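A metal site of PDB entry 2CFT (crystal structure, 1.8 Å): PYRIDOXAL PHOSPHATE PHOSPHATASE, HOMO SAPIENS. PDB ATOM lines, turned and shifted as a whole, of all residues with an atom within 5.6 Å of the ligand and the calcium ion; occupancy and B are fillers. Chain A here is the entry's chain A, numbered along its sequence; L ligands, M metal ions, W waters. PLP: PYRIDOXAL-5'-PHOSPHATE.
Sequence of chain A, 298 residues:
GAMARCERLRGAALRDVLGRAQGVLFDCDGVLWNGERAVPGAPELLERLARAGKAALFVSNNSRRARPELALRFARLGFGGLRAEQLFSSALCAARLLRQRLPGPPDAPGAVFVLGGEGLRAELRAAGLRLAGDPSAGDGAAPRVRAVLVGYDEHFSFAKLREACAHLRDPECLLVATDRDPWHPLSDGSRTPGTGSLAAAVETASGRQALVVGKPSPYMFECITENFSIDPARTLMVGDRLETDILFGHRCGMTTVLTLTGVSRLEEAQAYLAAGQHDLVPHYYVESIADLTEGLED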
ATOM      1  N   ASP A  27      10.644  37.283 -22.022  1.00  0.00           N
ATOM      2  CA  ASP A  27      10.710  36.109 -22.890  1.00  0.00           C
ATOM      3  C   ASP A  27      12.237  35.934 -23.179  1.00  0.00           C
ATOM      4  O   ASP A  27      13.031  36.865 -22.939  1.00  0.00           O
ATOM      5  CB  ASP A  27       9.861  36.444 -24.109  1.00  0.00           C
ATOM      6  CG  ASP A  27      10.124  35.572 -25.300  1.00  0.00           C
ATOM      7  OD1 ASP A  27      10.334  34.340 -25.155  1.00  0.00           O
ATOM      8  OD2 ASP A  27      10.007  36.138 -26.418  1.00  0.00           O
ATOM      9  N   CYS A  28      12.640  34.744 -23.617  1.00  0.00           N
ATOM     10  CA  CYS A  28      14.041  34.395 -23.700  1.00  0.00           C
ATOM     11  C   CYS A  28      14.543  34.333 -25.138  1.00  0.00           C
ATOM     12  O   CYS A  28      15.284  35.217 -25.585  1.00  0.00           O
ATOM     13  CB  CYS A  28      14.274  33.088 -22.922  1.00  0.00           C
ATOM     14  SG  CYS A  28      13.827  33.328 -21.162  1.00  0.00           S
ATOM     15  N   ASP A  29      14.112  33.336 -25.911  1.00  0.00           N
ATOM     16  CA  ASP A  29      14.649  33.226 -27.254  1.00  0.00           C
ATOM     17  C   ASP A  29      14.090  34.392 -28.085  1.00  0.00           C
ATOM     18  O   ASP A  29      12.903  34.745 -27.951  1.00  0.00           O
ATOM     19  CB  ASP A  29      14.245  31.903 -27.896  1.00  0.00           C
ATOM     20  CG  ASP A  29      14.758  31.793 -29.316  1.00  0.00           C
ATOM     21  OD1 ASP A  29      16.025  31.771 -29.469  1.00  0.00           O
ATOM     22  OD2 ASP A  29      13.914  31.851 -30.249  1.00  0.00           O
ATOM     23  N   GLY A  30      14.946  34.984 -28.915  1.00  0.00           N
ATOM     24  CA  GLY A  30      14.560  36.152 -29.721  1.00  0.00           C
ATOM     25  C   GLY A  30      14.678  37.474 -28.973  1.00  0.00           C
ATOM     26  O   GLY A  30      14.520  38.544 -29.564  1.00  0.00           O
ATOM     27  N   VAL A  31      15.016  37.409 -27.685  1.00  0.00           N
ATOM     28  CA  VAL A  31      14.972  38.577 -26.797  1.00  0.00           C
ATOM     29  C   VAL A  31      16.325  38.723 -26.128  1.00  0.00           C
ATOM     30  O   VAL A  31      17.014  39.714 -26.337  1.00  0.00           O
ATOM     31  CB  VAL A  31      13.882  38.430 -25.704  1.00  0.00           C
ATOM     32  CG1 VAL A  31      13.904  39.659 -24.719  1.00  0.00           C
ATOM     33  CG2 VAL A  31      12.495  38.264 -26.340  1.00  0.00           C
ATOM     34  N   VAL A  59      10.519  34.095 -18.655  1.00  0.00           N
ATOM     35  CA  VAL A  59       9.445  33.172 -18.997  1.00  0.00           C
ATOM     36  C   VAL A  59       9.659  32.618 -20.408  1.00  0.00           C
ATOM     37  O   VAL A  59       9.599  33.358 -21.395  1.00  0.00           O
ATOM     38  CB  VAL A  59       8.030  33.847 -18.848  1.00  0.00           C
ATOM     39  CG1 VAL A  59       7.933  35.181 -19.575  1.00  0.00           C
ATOM     40  CG2 VAL A  59       6.890  32.877 -19.218  1.00  0.00           C
ATOM     41  N   SER A  60       9.946  31.316 -20.477  1.00  0.00           N
ATOM     42  CA  SER A  60      10.206  30.659 -21.768  1.00  0.00           C
ATOM     43  C   SER A  60       9.251  29.495 -22.007  1.00  0.00           C
ATOM     44  O   SER A  60       9.025  28.699 -21.105  1.00  0.00           O
ATOM     45  CB  SER A  60      11.617  30.108 -21.785  1.00  0.00           C
ATOM     46  OG  SER A  60      11.947  29.549 -23.066  1.00  0.00           O
ATOM     47  N   ASN A  61       8.769  29.365 -23.247  1.00  0.00           N
ATOM     48  CA  ASN A  61       7.963  28.205 -23.637  1.00  0.00           C
ATOM     49  C   ASN A  61       8.806  26.960 -23.908  1.00  0.00           C
ATOM     50  O   ASN A  61       8.266  25.884 -24.238  1.00  0.00           O
ATOM     51  CB  ASN A  61       7.098  28.553 -24.869  1.00  0.00           C
ATOM     52  CG  ASN A  61       5.735  29.172 -24.454  1.00  0.00           C
ATOM     53  OD1 ASN A  61       5.466  29.311 -23.260  1.00  0.00           O
ATOM     54  ND2 ASN A  61       4.941  29.598 -25.432  1.00  0.00           N
ATOM     55  N   ASN A  62      10.115  27.091 -23.769  1.00  0.00           N
ATOM     56  CA  ASN A  62      11.019  25.998 -24.106  1.00  0.00           C
ATOM     57  C   ASN A  62      10.791  24.864 -23.115  1.00  0.00           C
ATOM     58  O   ASN A  62      10.957  25.069 -21.910  1.00  0.00           O
ATOM     59  CB  ASN A  62      12.480  26.463 -24.084  1.00  0.00           C
ATOM     60  CG  ASN A  62      13.396  25.551 -24.890  1.00  0.00           C
ATOM     61  OD1 ASN A  62      13.223  24.343 -24.884  1.00  0.00           O
ATOM     62  ND2 ASN A  62      14.365  26.131 -25.613  1.00  0.00           N
ATOM     63  N   SER A  63      10.373  23.704 -23.620  1.00  0.00           N
ATOM     64  CA  SER A  63      10.155  22.517 -22.784  1.00  0.00           C
ATOM     65  C   SER A  63      11.347  21.559 -22.816  1.00  0.00           C
ATOM     66  O   SER A  63      11.239  20.449 -22.343  1.00  0.00           O
ATOM     67  CB  SER A  63       8.895  21.760 -23.246  1.00  0.00           C
ATOM     68  OG  SER A  63       8.964  21.431 -24.640  1.00  0.00           O
ATOM     69  N   ARG A  64      12.479  21.986 -23.364  1.00  0.00           N
ATOM     70  CA  ARG A  64      13.639  21.068 -23.485  1.00  0.00           C
ATOM     71  C   ARG A  64      14.411  20.870 -22.198  1.00  0.00           C
ATOM     72  O   ARG A  64      14.943  19.788 -21.972  1.00  0.00           O
ATOM     73  CB  ARG A  64      14.624  21.509 -24.565  1.00  0.00           C
ATOM     74  CG  ARG A  64      14.293  20.964 -25.942  1.00  0.00           C
ATOM     75  CD  ARG A  64      15.356  21.388 -26.929  1.00  0.00           C
ATOM     76  NE  ARG A  64      15.696  20.343 -27.882  1.00  0.00           N
ATOM     77  CZ  ARG A  64      16.518  19.324 -27.646  1.00  0.00           C
ATOM     78  NH1 ARG A  64      17.104  19.196 -26.454  1.00  0.00           N
ATOM     79  NH2 ARG A  64      16.753  18.425 -28.578  1.00  0.00           N
ATOM     80  N   ARG A  73      22.302  27.517 -18.779  1.00  0.00           N
ATOM     81  CA  ARG A  73      22.219  28.230 -20.063  1.00  0.00           C
ATOM     82  C   ARG A  73      22.219  29.765 -19.927  1.00  0.00           C
ATOM     83  O   ARG A  73      22.909  30.470 -20.666  1.00  0.00           O
ATOM     84  CB  ARG A  73      21.015  27.735 -20.881  1.00  0.00           C
ATOM     85  CG  ARG A  73      20.803  28.508 -22.204  1.00  0.00           C
ATOM     86  CD  ARG A  73      19.747  27.808 -23.044  1.00  0.00           C
ATOM     87  NE  ARG A  73      19.309  28.571 -24.240  1.00  0.00           N
ATOM     88  CZ  ARG A  73      20.047  28.693 -25.343  1.00  0.00           C
ATOM     89  NH1 ARG A  73      21.247  28.152 -25.411  1.00  0.00           N
ATOM     90  NH2 ARG A  73      19.581  29.380 -26.395  1.00  0.00           N
ATOM     91  N   TYR A 152       7.814  19.311 -26.515  1.00  0.00           N
ATOM     92  CA  TYR A 152       8.682  19.229 -27.688  1.00  0.00           C
ATOM     93  C   TYR A 152       9.303  17.830 -27.703  1.00  0.00           C
ATOM     94  O   TYR A 152      10.075  17.455 -26.803  1.00  0.00           O
ATOM     95  CB  TYR A 152       9.747  20.320 -27.608  1.00  0.00           C
ATOM     96  CG  TYR A 152      10.700  20.279 -28.781  1.00  0.00           C
ATOM     97  CD1 TYR A 152      10.385  20.904 -29.989  1.00  0.00           C
ATOM     98  CD2 TYR A 152      11.936  19.651 -28.655  1.00  0.00           C
ATOM     99  CE1 TYR A 152      11.274  20.879 -31.057  1.00  0.00           C
ATOM    100  CE2 TYR A 152      12.835  19.625 -29.744  1.00  0.00           C
ATOM    101  CZ  TYR A 152      12.490  20.242 -30.921  1.00  0.00           C
ATOM    102  OH  TYR A 152      13.370  20.250 -31.977  1.00  0.00           O
ATOM    103  N   ASP A 179       3.023  24.113 -24.816  1.00  0.00           N
ATOM    104  CA  ASP A 179       2.924  25.367 -25.548  1.00  0.00           C
ATOM    105  C   ASP A 179       2.407  25.074 -26.947  1.00  0.00           C
ATOM    106  O   ASP A 179       2.335  23.902 -27.339  1.00  0.00           O
ATOM    107  CB  ASP A 179       4.321  26.035 -25.643  1.00  0.00           C
ATOM    108  CG  ASP A 179       5.315  25.234 -26.490  1.00  0.00           C
ATOM    109  OD1 ASP A 179       5.472  25.555 -27.719  1.00  0.00           O
ATOM    110  OD2 ASP A 179       5.893  24.237 -25.995  1.00  0.00           O
ATOM    111  N   ASP A 181       3.759  26.937 -29.681  1.00  0.00           N
ATOM    112  CA  ASP A 181       4.644  27.604 -30.654  1.00  0.00           C
ATOM    113  C   ASP A 181       4.759  26.693 -31.891  1.00  0.00           C
ATOM    114  O   ASP A 181       5.075  25.504 -31.750  1.00  0.00           O
ATOM    115  CB  ASP A 181       6.061  27.851 -30.102  1.00  0.00           C
ATOM    116  CG  ASP A 181       6.084  28.833 -28.890  1.00  0.00           C
ATOM    117  OD1 ASP A 181       7.182  29.077 -28.363  1.00  0.00           O
ATOM    118  OD2 ASP A 181       5.024  29.329 -28.498  1.00  0.00           O
ATOM    119  N   HIS A 184      10.395  26.940 -34.609  1.00  0.00           N
ATOM    120  CA  HIS A 184      11.432  27.863 -34.073  1.00  0.00           C
ATOM    121  C   HIS A 184      12.568  27.995 -35.047  1.00  0.00           C
ATOM    122  O   HIS A 184      13.029  26.981 -35.586  1.00  0.00           O
ATOM    123  CB  HIS A 184      11.976  27.340 -32.755  1.00  0.00           C
ATOM    124  CG  HIS A 184      10.889  27.040 -31.764  1.00  0.00           C
ATOM    125  ND1 HIS A 184      10.291  28.046 -31.034  1.00  0.00           N
ATOM    126  CD2 HIS A 184      10.246  25.895 -31.453  1.00  0.00           C
ATOM    127  CE1 HIS A 184       9.330  27.514 -30.281  1.00  0.00           C
ATOM    128  NE2 HIS A 184       9.301  26.210 -30.508  1.00  0.00           N
ATOM    129  N   THR A 192      12.893  24.347 -36.791  1.00  0.00           N
ATOM    130  CA  THR A 192      12.519  23.069 -36.204  1.00  0.00           C
ATOM    131  C   THR A 192      11.014  23.157 -35.919  1.00  0.00           C
ATOM    132  O   THR A 192      10.521  24.218 -35.511  1.00  0.00           O
ATOM    133  CB  THR A 192      13.320  22.702 -34.931  1.00  0.00           C
ATOM    134  OG1 THR A 192      13.064  21.342 -34.583  1.00  0.00           O
ATOM    135  CG2 THR A 192      12.935  23.565 -33.738  1.00  0.00           C
ATOM    136  N   THR A 195       6.208  22.579 -30.559  1.00  0.00           N
ATOM    137  CA  THR A 195       5.220  21.762 -29.858  1.00  0.00           C
ATOM    138  C   THR A 195       3.820  21.959 -30.464  1.00  0.00           C
ATOM    139  O   THR A 195       3.016  21.027 -30.467  1.00  0.00           O
ATOM    140  CB  THR A 195       5.217  22.085 -28.338  1.00  0.00           C
ATOM    141  OG1 THR A 195       6.529  21.885 -27.815  1.00  0.00           O
ATOM    142  CG2 THR A 195       4.237  21.191 -27.590  1.00  0.00           C
ATOM    143  N   LYS A 215       2.910  30.418 -22.394  1.00  0.00           N
ATOM    144  CA  LYS A 215       2.413  31.616 -23.081  1.00  0.00           C
ATOM    145  C   LYS A 215       1.701  31.201 -24.389  1.00  0.00           C
ATOM    146  O   LYS A 215       2.202  30.319 -25.116  1.00  0.00           O
ATOM    147  CB  LYS A 215       3.612  32.515 -23.459  1.00  0.00           C
ATOM    148  CG  LYS A 215       4.559  32.791 -22.277  1.00  0.00           C
ATOM    149  CD  LYS A 215       5.813  33.566 -22.783  1.00  0.00           C
ATOM    150  CE  LYS A 215       6.752  32.648 -23.570  1.00  0.00           C
ATOM    151  NZ  LYS A 215       8.022  33.365 -24.004  1.00  0.00           N
ATOM    152  N   ASP A 240       9.361  38.546 -28.386  1.00  0.00           N
ATOM    153  CA  ASP A 240       9.557  38.660 -29.831  1.00  0.00           C
ATOM    154  C   ASP A 240       8.419  38.050 -30.666  1.00  0.00           C
ATOM    155  O   ASP A 240       8.485  38.095 -31.900  1.00  0.00           O
ATOM    156  CB  ASP A 240      10.876  37.980 -30.248  1.00  0.00           C
ATOM    157  CG  ASP A 240      10.767  36.444 -30.207  1.00  0.00           C
ATOM    158  OD1 ASP A 240      10.144  35.938 -29.255  1.00  0.00           O
ATOM    159  OD2 ASP A 240      11.320  35.755 -31.093  1.00  0.00           O
ATOM    160  N   ARG A 241       7.403  37.456 -30.033  1.00  0.00           N
ATOM    161  CA  ARG A 241       6.346  36.792 -30.792  1.00  0.00           C
ATOM    162  C   ARG A 241       4.969  37.417 -30.483  1.00  0.00           C
ATOM    163  O   ARG A 241       4.524  37.393 -29.342  1.00  0.00           O
ATOM    164  CB  ARG A 241       6.360  35.267 -30.464  1.00  0.00           C
ATOM    165  CG  ARG A 241       7.357  34.414 -31.281  1.00  0.00           C
ATOM    166  CD  ARG A 241       7.017  32.886 -31.286  1.00  0.00           C
ATOM    167  NE  ARG A 241       6.583  32.317 -32.584  1.00  0.00           N
ATOM    168  CZ  ARG A 241       7.136  31.241 -33.161  1.00  0.00           C
ATOM    169  NH1 ARG A 241       8.112  30.598 -32.534  1.00  0.00           N
ATOM    170  NH2 ARG A 241       6.713  30.770 -34.349  1.00  0.00           N
ATOM    171  N   ASP A 245       3.962  36.162 -26.864  1.00  0.00           N
ATOM    172  CA  ASP A 245       4.335  37.060 -25.770  1.00  0.00           C
ATOM    173  C   ASP A 245       3.484  38.302 -25.668  1.00  0.00           C
ATOM    174  O   ASP A 245       3.209  38.775 -24.551  1.00  0.00           O
ATOM    175  CB  ASP A 245       5.785  37.486 -25.964  1.00  0.00           C
ATOM    176  CG  ASP A 245       6.662  36.313 -26.249  1.00  0.00           C
ATOM    177  OD1 ASP A 245       6.881  35.536 -25.302  1.00  0.00           O
ATOM    178  OD2 ASP A 245       7.054  36.116 -27.417  1.00  0.00           O
HETATM  179  N1  PLP L   1      10.478  25.626 -27.468  1.00  0.00           N
HETATM  180  C2  PLP L   1      11.513  25.016 -28.139  1.00  0.00           C
HETATM  181  C2A PLP L   1      11.465  23.534 -28.394  1.00  0.00           C
HETATM  182  C3  PLP L   1      12.610  25.761 -28.593  1.00  0.00           C
HETATM  183  O3  PLP L   1      13.732  25.132 -29.077  1.00  0.00           O
HETATM  184  C4  PLP L   1      12.654  27.128 -28.371  1.00  0.00           C
HETATM  185  C4A PLP L   1      13.849  27.940 -28.795  1.00  0.00           C
HETATM  186  O4A PLP L   1      14.957  27.395 -28.795  1.00  0.00           O
HETATM  187  C5  PLP L   1      11.621  27.759 -27.706  1.00  0.00           C
HETATM  188  C6  PLP L   1      10.533  27.004 -27.234  1.00  0.00           C
HETATM  189  C5A PLP L   1      11.962  29.177 -27.226  1.00  0.00           C
HETATM  190  O4P PLP L   1      10.939  29.625 -26.385  1.00  0.00           O
HETATM  191  P   PLP L   1      10.903  31.143 -25.893  1.00  0.00           P
HETATM  192  O1P PLP L   1      10.959  32.014 -27.121  1.00  0.00           O
HETATM  193  O2P PLP L   1      12.051  31.410 -24.927  1.00  0.00           O
HETATM  194  O3P PLP L   1       9.533  31.231 -25.256  1.00  0.00           O
HETATM  195 CA    CA M   1      10.608  34.141 -27.791  1.00  0.00          CA
HETATM  196  O   HOH W   1       7.394  31.413 -26.884  1.00  0.00           O
HETATM  197  O   HOH W   2       9.405  30.776 -29.472  1.00  0.00           O
HETATM  198  O   HOH W   3      10.934  33.237 -30.013  1.00  0.00           O
HETATM  199  O   HOH W   4       8.570  23.673 -26.188  1.00  0.00           O
HETATM  200  O   HOH W   5       8.274  33.678 -27.855  1.00  0.00           O
HETATM  201  O   HOH W   6      17.200  28.988 -28.739  1.00  0.00           O
HETATM  202  O   HOH W   7      15.041  28.871 -31.548  1.00  0.00           O
HETATM  203  O   HOH W   8       7.621  24.504 -29.009  1.00  0.00           O
HETATM  204  O   HOH W   9      16.910  25.208 -27.257  1.00  0.00           O
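The calcium ion is bound by O1P of the ligand (2.3 Å), OD1 of Asp 240 (2.4 Å), O of Asp 29 (2.4 Å), water W5 (2.4 Å), water W3 (2.4 Å), OD2 of Asp 27 (2.5 Å) and OD1 of Asp 27 (2.7 Å). The calcium ion has seven donor atoms within binding distance.
Cys 28 touches the ligand. CD1 of Tyr 152 touches C2A of the ligand, 3.3 Å away. Of the 22 residues printed, 9 come within 4 Å of the ligand. The nearest printed residue that does not touch the ligand is Asp 181 (4.1 Å).
Of the 22 residues printed, 3 come within 4 Å of the calcium ion.
Water W3 lies within hydrogen-bond range of the side-chain carboxylate (OD2) of Asp 240 (2.8 Å) and the side-chain carboxylate (OD2) of Asp 29 (3.3 Å). Water W1 lies within hydrogen-bond range of O3P of the ligand, OD1 of Asp 181 and ND2 of Asn 61. Water W6 lies within hydrogen-bond range of an oxygen (O4A) of the ligand (2.8 Å), the side-chain carboxylate of Asp 29 (3.1 Å) and the guanidinium group of Arg 73 (3.4 Å). Water W7 bridges O4A of the ligand (3.1 Å) and OD2 of Asp 29 (3.4 Å). Water W9 lies within hydrogen-bond range of ND2 of Asn 62 (3.2 Å) and O4A of the ligand (3.3 Å). Water W8 lies within hydrogen-bond range of the side-chain carboxylate (OD1) of Asp 179 (2.7 Å), a ring nitrogen (NE2) of His 184 (2.8 Å), the backbone NH (N) of Thr 195 (2.8 Å) and a nitrogen (N1) of the ligand (3.4 Å).
N of Asp 29 sits at hydrogen-bond distance from O2P of the ligand, 3.0 Å away. The side-chain hydroxyl (OG) of Ser 60 is in hydrogen-bond range of an oxygen (O2P) of the ligand (2.6 Å). An oxygen (O3P) of the ligand lies within hydrogen-bond range of the backbone NH of Asn 61 (2.8 Å). An oxygen (O3P) of the ligand lies within salt-bridge range of the side-chain amino group of Lys 215 (2.9 Å). A ring nitrogen (NE2) of His 184 is in hydrogen-bond range of a nitrogen (N1) of the ligand (3.3 Å). The side-chain amide nitrogen (ND2) of Asn 62 sits close to an oxygen (O4A) of the ligand, at 3.5 Å.
OD2 of Asp 245 sits at hydrogen-bond distance from N of Asp 240, 3.5 Å away. The side-chain amino group of Lys 215 sits close to the side-chain carboxylate of Asp 27, at 2.8 Å. The backbone NH (N) of Asn 62 sits close to the side-chain hydroxyl (OG) of Ser 60 (3.1 Å). The backbone carbonyl oxygen (O) of Lys 215 sits at hydrogen-bond distance from the side-chain amide nitrogen (ND2) of Asn 61, at 2.8 Å. The side-chain amino group of Lys 215 is in salt-bridge range of the side-chain carboxylate of Asp 245 (2.8 Å). The backbone NH of Tyr 152 is in hydrogen-bond range of the side-chain hydroxyl of Ser 63 (3.1 Å). The side-chain hydroxyl of Thr 192 is in hydrogen-bond range of the side-chain hydroxyl of Tyr 152 (2.8 Å). The backbone carbonyl oxygen of Thr 192 sits at hydrogen-bond distance from the backbone NH of His 184.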
